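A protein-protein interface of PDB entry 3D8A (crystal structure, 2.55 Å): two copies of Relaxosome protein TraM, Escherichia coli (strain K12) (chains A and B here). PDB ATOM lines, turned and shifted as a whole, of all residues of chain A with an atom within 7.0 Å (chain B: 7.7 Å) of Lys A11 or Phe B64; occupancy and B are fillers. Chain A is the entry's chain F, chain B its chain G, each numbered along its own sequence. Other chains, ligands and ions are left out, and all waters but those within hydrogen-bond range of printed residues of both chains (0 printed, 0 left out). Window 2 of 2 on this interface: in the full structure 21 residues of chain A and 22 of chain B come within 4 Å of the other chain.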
ATOM      1  N   GLN A   6     -15.410   1.487  -5.172  1.00  0.00           N
ATOM      2  CA  GLN A   6     -15.102   2.804  -5.743  1.00  0.00           C
ATOM      3  C   GLN A   6     -13.663   2.917  -6.255  1.00  0.00           C
ATOM      4  O   GLN A   6     -13.419   3.597  -7.256  1.00  0.00           O
ATOM      5  CB  GLN A   6     -15.436   3.940  -4.762  1.00  0.00           C
ATOM      6  CG  GLN A   6     -15.346   5.362  -5.358  1.00  0.00           C
ATOM      7  CD  GLN A   6     -16.382   5.641  -6.443  1.00  0.00           C
ATOM      8  OE1 GLN A   6     -17.585   5.521  -6.215  1.00  0.00           O
ATOM      9  NE2 GLN A   6     -15.913   6.022  -7.628  1.00  0.00           N
ATOM     10  N   THR A   7     -12.728   2.235  -5.591  1.00  0.00           N
ATOM     11  CA  THR A   7     -11.324   2.235  -6.011  1.00  0.00           C
ATOM     12  C   THR A   7     -11.148   1.558  -7.366  1.00  0.00           C
ATOM     13  O   THR A   7     -10.488   2.110  -8.252  1.00  0.00           O
ATOM     14  CB  THR A   7     -10.392   1.576  -4.967  1.00  0.00           C
ATOM     15  OG1 THR A   7     -10.736   2.035  -3.653  1.00  0.00           O
ATOM     16  CG2 THR A   7      -8.935   1.915  -5.254  1.00  0.00           C
ATOM     17  N   GLU A   8     -11.746   0.378  -7.532  1.00  0.00           N
ATOM     18  CA  GLU A   8     -11.686  -0.349  -8.804  1.00  0.00           C
ATOM     19  C   GLU A   8     -12.385   0.425  -9.925  1.00  0.00           C
ATOM     20  O   GLU A   8     -11.930   0.416 -11.070  1.00  0.00           O
ATOM     21  CB  GLU A   8     -12.260  -1.765  -8.664  1.00  0.00           C
ATOM     22  CG  GLU A   8     -11.504  -2.675  -7.681  1.00  0.00           C
ATOM     23  CD  GLU A   8     -10.057  -2.982  -8.094  1.00  0.00           C
ATOM     24  OE1 GLU A   8      -9.727  -2.929  -9.304  1.00  0.00           O
ATOM     25  OE2 GLU A   8      -9.245  -3.289  -7.193  1.00  0.00           O
ATOM     26  N   PHE A   9     -13.481   1.095  -9.577  1.00  0.00           N
ATOM     27  CA  PHE A   9     -14.217   1.940 -10.512  1.00  0.00           C
ATOM     28  C   PHE A   9     -13.327   3.071 -11.017  1.00  0.00           C
ATOM     29  O   PHE A   9     -13.241   3.309 -12.214  1.00  0.00           O
ATOM     30  CB  PHE A   9     -15.476   2.504  -9.844  1.00  0.00           C
ATOM     31  CG  PHE A   9     -16.377   3.244 -10.786  1.00  0.00           C
ATOM     32  CD1 PHE A   9     -16.287   4.635 -10.904  1.00  0.00           C
ATOM     33  CD2 PHE A   9     -17.311   2.556 -11.563  1.00  0.00           C
ATOM     34  CE1 PHE A   9     -17.121   5.335 -11.779  1.00  0.00           C
ATOM     35  CE2 PHE A   9     -18.148   3.239 -12.441  1.00  0.00           C
ATOM     36  CZ  PHE A   9     -18.053   4.632 -12.554  1.00  0.00           C
ATOM     37  N   ASN A  10     -12.654   3.749 -10.094  1.00  0.00           N
ATOM     38  CA  ASN A  10     -11.704   4.802 -10.445  1.00  0.00           C
ATOM     39  C   ASN A  10     -10.539   4.317 -11.315  1.00  0.00           C
ATOM     40  O   ASN A  10     -10.119   5.026 -12.234  1.00  0.00           O
ATOM     41  CB  ASN A  10     -11.186   5.507  -9.183  1.00  0.00           C
ATOM     42  CG  ASN A  10     -12.242   6.387  -8.522  1.00  0.00           C
ATOM     43  OD1 ASN A  10     -12.056   6.856  -7.398  1.00  0.00           O
ATOM     44  ND2 ASN A  10     -13.355   6.609  -9.210  1.00  0.00           N
ATOM     45  N   LYS A  11     -10.034   3.115 -11.025  1.00  0.00           N
ATOM     46  CA  LYS A  11      -8.965   2.498 -11.819  1.00  0.00           C
ATOM     47  C   LYS A  11      -9.383   2.306 -13.266  1.00  0.00           C
ATOM     48  O   LYS A  11      -8.682   2.750 -14.171  1.00  0.00           O
ATOM     49  CB  LYS A  11      -8.503   1.160 -11.221  1.00  0.00           C
ATOM     50  CG  LYS A  11      -7.197   1.262 -10.466  1.00  0.00           C
ATOM     51  CD  LYS A  11      -6.610  -0.099 -10.071  1.00  0.00           C
ATOM     52  CE  LYS A  11      -5.587  -0.589 -11.092  1.00  0.00           C
ATOM     53  NZ  LYS A  11      -4.769  -1.719 -10.557  1.00  0.00           N
ATOM     54  N   LEU A  12     -10.526   1.654 -13.467  1.00  0.00           N
ATOM     55  CA  LEU A  12     -11.052   1.418 -14.801  1.00  0.00           C
ATOM     56  C   LEU A  12     -11.353   2.730 -15.506  1.00  0.00           C
ATOM     57  O   LEU A  12     -10.958   2.927 -16.648  1.00  0.00           O
ATOM     58  CB  LEU A  12     -12.306   0.546 -14.745  1.00  0.00           C
ATOM     59  CG  LEU A  12     -12.688  -0.084 -16.088  1.00  0.00           C
ATOM     60  CD1 LEU A  12     -11.598  -1.041 -16.555  1.00  0.00           C
ATOM     61  CD2 LEU A  12     -14.014  -0.810 -15.979  1.00  0.00           C
ATOM     62  N   LEU A  13     -12.040   3.630 -14.807  1.00  0.00           N
ATOM     63  CA  LEU A  13     -12.379   4.939 -15.351  1.00  0.00           C
ATOM     64  C   LEU A  13     -11.139   5.688 -15.833  1.00  0.00           C
ATOM     65  O   LEU A  13     -11.107   6.151 -16.978  1.00  0.00           O
ATOM     66  CB  LEU A  13     -13.182   5.770 -14.338  1.00  0.00           C
ATOM     67  CG  LEU A  13     -13.671   7.144 -14.807  1.00  0.00           C
ATOM     68  CD1 LEU A  13     -14.761   7.005 -15.882  1.00  0.00           C
ATOM     69  CD2 LEU A  13     -14.153   7.981 -13.647  1.00  0.00           C
ATOM     70  N   LEU A  14     -10.115   5.772 -14.988  1.00  0.00           N
ATOM     71  CA  LEU A  14      -8.876   6.446 -15.372  1.00  0.00           C
ATOM     72  C   LEU A  14      -8.142   5.739 -16.520  1.00  0.00           C
ATOM     73  O   LEU A  14      -7.687   6.395 -17.457  1.00  0.00           O
ATOM     74  CB  LEU A  14      -7.956   6.666 -14.163  1.00  0.00           C
ATOM     75  CG  LEU A  14      -6.942   7.812 -14.332  1.00  0.00           C
ATOM     76  CD1 LEU A  14      -7.630   9.166 -14.591  1.00  0.00           C
ATOM     77  CD2 LEU A  14      -6.002   7.905 -13.130  1.00  0.00           C
ATOM     78  N   GLU A  15      -8.051   4.412 -16.459  1.00  0.00           N
ATOM     79  CA  GLU A  15      -7.430   3.633 -17.527  1.00  0.00           C
ATOM     80  C   GLU A  15      -8.071   3.930 -18.893  1.00  0.00           C
ATOM     81  O   GLU A  15      -7.372   4.123 -19.896  1.00  0.00           O
ATOM     82  CB  GLU A  15      -7.499   2.136 -17.206  1.00  0.00           C
ATOM     83  CG  GLU A  15      -7.502   1.224 -18.429  1.00  0.00           C
ATOM     84  CD  GLU A  15      -7.072  -0.199 -18.131  1.00  0.00           C
ATOM     85  OE1 GLU A  15      -7.497  -0.763 -17.094  1.00  0.00           O
ATOM     86  OE2 GLU A  15      -6.312  -0.759 -18.956  1.00  0.00           O
ATOM     87  N   CYS A  16      -9.400   3.981 -18.918  1.00  0.00           N
ATOM     88  CA  CYS A  16     -10.132   4.221 -20.151  1.00  0.00           C
ATOM     89  C   CYS A  16      -9.880   5.604 -20.719  1.00  0.00           C
ATOM     90  O   CYS A  16      -9.595   5.736 -21.894  1.00  0.00           O
ATOM     91  CB  CYS A  16     -11.619   4.008 -19.936  1.00  0.00           C
ATOM     92  SG  CYS A  16     -12.041   2.279 -19.743  1.00  0.00           S
ATOM     93  N   LEU B  14     -19.522   4.903 -16.928  1.00  0.00           N
ATOM     94  CA  LEU B  14     -18.714   3.732 -17.248  1.00  0.00           C
ATOM     95  C   LEU B  14     -19.029   3.152 -18.626  1.00  0.00           C
ATOM     96  O   LEU B  14     -18.109   2.809 -19.363  1.00  0.00           O
ATOM     97  CB  LEU B  14     -18.831   2.653 -16.167  1.00  0.00           C
ATOM     98  CG  LEU B  14     -17.743   1.574 -16.169  1.00  0.00           C
ATOM     99  CD1 LEU B  14     -16.342   2.177 -15.953  1.00  0.00           C
ATOM    100  CD2 LEU B  14     -18.037   0.497 -15.139  1.00  0.00           C
ATOM    101  N   VAL B  56      -0.221   5.193 -20.518  1.00  0.00           N
ATOM    102  CA  VAL B  56      -1.210   4.751 -19.534  1.00  0.00           C
ATOM    103  C   VAL B  56      -0.532   4.351 -18.233  1.00  0.00           C
ATOM    104  O   VAL B  56      -0.924   4.814 -17.164  1.00  0.00           O
ATOM    105  CB  VAL B  56      -2.066   3.577 -20.078  1.00  0.00           C
ATOM    106  CG1 VAL B  56      -2.866   2.896 -18.964  1.00  0.00           C
ATOM    107  CG2 VAL B  56      -2.992   4.067 -21.184  1.00  0.00           C
ATOM    108  N   SER B  57       0.500   3.512 -18.337  1.00  0.00           N
ATOM    109  CA  SER B  57       1.248   3.042 -17.173  1.00  0.00           C
ATOM    110  C   SER B  57       1.745   4.187 -16.302  1.00  0.00           C
ATOM    111  O   SER B  57       1.583   4.141 -15.086  1.00  0.00           O
ATOM    112  CB  SER B  57       2.415   2.149 -17.593  1.00  0.00           C
ATOM    113  OG  SER B  57       1.986   1.190 -18.546  1.00  0.00           O
ATOM    114  N   GLU B  59       0.677   7.294 -16.110  1.00  0.00           N
ATOM    115  CA  GLU B  59      -0.439   8.009 -15.510  1.00  0.00           C
ATOM    116  C   GLU B  59      -1.100   7.191 -14.406  1.00  0.00           C
ATOM    117  O   GLU B  59      -1.510   7.748 -13.384  1.00  0.00           O
ATOM    118  CB  GLU B  59      -1.482   8.405 -16.562  1.00  0.00           C
ATOM    119  CG  GLU B  59      -0.965   9.347 -17.649  1.00  0.00           C
ATOM    120  CD  GLU B  59      -0.564  10.735 -17.144  1.00  0.00           C
ATOM    121  OE1 GLU B  59      -0.621  10.999 -15.920  1.00  0.00           O
ATOM    122  OE2 GLU B  59      -0.181  11.570 -17.989  1.00  0.00           O
ATOM    123  N   MET B  60      -1.209   5.877 -14.614  1.00  0.00           N
ATOM    124  CA  MET B  60      -1.810   4.987 -13.615  1.00  0.00           C
ATOM    125  C   MET B  60      -0.925   4.844 -12.370  1.00  0.00           C
ATOM    126  O   MET B  60      -1.424   4.916 -11.244  1.00  0.00           O
ATOM    127  CB  MET B  60      -2.151   3.618 -14.212  1.00  0.00           C
ATOM    128  CG  MET B  60      -3.239   3.641 -15.297  1.00  0.00           C
ATOM    129  SD  MET B  60      -4.919   4.046 -14.747  1.00  0.00           S
ATOM    130  CE  MET B  60      -5.326   2.572 -13.807  1.00  0.00           C
ATOM    131  N   GLU B  61       0.378   4.656 -12.589  1.00  0.00           N
ATOM    132  CA  GLU B  61       1.380   4.522 -11.514  1.00  0.00           C
ATOM    133  C   GLU B  61       1.319   5.702 -10.538  1.00  0.00           C
ATOM    134  O   GLU B  61       1.574   5.553  -9.342  1.00  0.00           O
ATOM    135  CB  GLU B  61       2.790   4.388 -12.123  1.00  0.00           C
ATOM    136  CG  GLU B  61       3.950   4.215 -11.129  1.00  0.00           C
ATOM    137  CD  GLU B  61       4.170   2.774 -10.666  1.00  0.00           C
ATOM    138  OE1 GLU B  61       3.450   1.860 -11.125  1.00  0.00           O
ATOM    139  OE2 GLU B  61       5.077   2.554  -9.836  1.00  0.00           O
ATOM    140  N   ARG B  62       0.964   6.864 -11.074  1.00  0.00           N
ATOM    141  CA  ARG B  62       0.794   8.101 -10.324  1.00  0.00           C
ATOM    142  C   ARG B  62      -0.330   8.020  -9.277  1.00  0.00           C
ATOM    143  O   ARG B  62      -0.206   8.590  -8.187  1.00  0.00           O
ATOM    144  CB  ARG B  62       0.516   9.234 -11.317  1.00  0.00           C
ATOM    145  CG  ARG B  62       0.731  10.625 -10.781  1.00  0.00           C
ATOM    146  CD  ARG B  62       0.253  11.648 -11.787  1.00  0.00           C
ATOM    147  NE  ARG B  62      -0.184  12.865 -11.113  1.00  0.00           N
ATOM    148  CZ  ARG B  62      -0.784  13.887 -11.712  1.00  0.00           C
ATOM    149  NH1 ARG B  62      -1.027  13.855 -13.017  1.00  0.00           N
ATOM    150  NH2 ARG B  62      -1.141  14.944 -10.996  1.00  0.00           N
ATOM    151  N   PHE B  63      -1.414   7.315  -9.609  1.00  0.00           N
ATOM    152  CA  PHE B  63      -2.583   7.210  -8.721  1.00  0.00           C
ATOM    153  C   PHE B  63      -2.790   5.840  -8.059  1.00  0.00           C
ATOM    154  O   PHE B  63      -3.522   5.735  -7.070  1.00  0.00           O
ATOM    155  CB  PHE B  63      -3.862   7.645  -9.454  1.00  0.00           C
ATOM    156  CG  PHE B  63      -3.915   9.111  -9.753  1.00  0.00           C
ATOM    157  CD1 PHE B  63      -4.384  10.008  -8.803  1.00  0.00           C
ATOM    158  CD2 PHE B  63      -3.482   9.599 -10.977  1.00  0.00           C
ATOM    159  CE1 PHE B  63      -4.424  11.368  -9.072  1.00  0.00           C
ATOM    160  CE2 PHE B  63      -3.518  10.954 -11.256  1.00  0.00           C
ATOM    161  CZ  PHE B  63      -3.992  11.842 -10.303  1.00  0.00           C
ATOM    162  N   PHE B  64      -2.151   4.800  -8.600  1.00  0.00           N
ATOM    163  CA  PHE B  64      -2.330   3.432  -8.101  1.00  0.00           C
ATOM    164  C   PHE B  64      -1.028   2.627  -8.061  1.00  0.00           C
ATOM    165  O   PHE B  64      -0.436   2.372  -9.108  1.00  0.00           O
ATOM    166  CB  PHE B  64      -3.384   2.698  -8.937  1.00  0.00           C
ATOM    167  CG  PHE B  64      -4.702   3.413  -9.009  1.00  0.00           C
ATOM    168  CD1 PHE B  64      -5.629   3.298  -7.974  1.00  0.00           C
ATOM    169  CD2 PHE B  64      -5.013   4.221 -10.104  1.00  0.00           C
ATOM    170  CE1 PHE B  64      -6.850   3.964  -8.032  1.00  0.00           C
ATOM    171  CE2 PHE B  64      -6.231   4.895 -10.172  1.00  0.00           C
ATOM    172  CZ  PHE B  64      -7.153   4.764  -9.133  1.00  0.00           C
ATOM    173  N   PRO B  65      -0.572   2.236  -6.846  1.00  0.00           N
ATOM    174  CA  PRO B  65       0.608   1.372  -6.702  1.00  0.00           C
ATOM    175  C   PRO B  65       0.339  -0.054  -7.176  1.00  0.00           C
ATOM    176  O   PRO B  65       0.483  -0.345  -8.363  1.00  0.00           O
ATOM    177  CB  PRO B  65       0.881   1.381  -5.185  1.00  0.00           C
ATOM    178  CG  PRO B  65       0.071   2.515  -4.636  1.00  0.00           C
ATOM    179  CD  PRO B  65      -1.123   2.612  -5.534  1.00  0.00           C
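N of Glu A15 sits at hydrogen-bond distance from SD of Met B60.
The side-chain sulfur (SG) of Cys A16 sits at hydrogen-bond distance from the backbone carbonyl oxygen (O) of Leu A12 (3.3 Å).
Phe A9 touches Leu B14. Met B60 touches Lys A11 (CE to O, 3.4 Å). Lys A11 touches Phe B64. Leu A12 touches Leu B14 (CD2 to CD1, 3.8 Å). CD2 of Leu A14 touches CD2 of Phe B63 (3.7 Å).
Of chain B, only Met B60 and Phe B64 come within 4 Å of Lys A11. Phe B64 touches just one residue of chain A: Lys A11. Of the printed residues of chain A, Met B60 touches Lys A11 and Glu A15. Printed residues of chain B within 4 Å of Phe A9: Leu B14 (3.8 Å). Of the printed residues of chain A, Leu B14 touches Phe A9 and Leu A12. Of the printed residues of chain A, Phe B63 touches Leu A14 (3.7 Å). The nearest residue of chain B that does not touch Lys A11 is Pro B65 (5.9 Å).
Hydrophobic or aromatic side chains of chain B that line the printed part of chain A: Leu B14, Met B60, Phe B63 and Phe B64. Of the 11 printed residues of chain A, 5 touch a printed residue of chain B. Hydrophobic or aromatic side chains of chain A within 4 Å of the printed part of chain B: Phe A9, Leu A12 and Leu A14. Among the printed residues, no Asp or Glu carboxylate lies within 4 Å of a Lys or Arg side-chain nitrogen of the other chain.
Position printed for both chains: 14. Of the 6 pairs that touch across the chains among the printed residues, none has its exchanged pair printed and touching as well.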
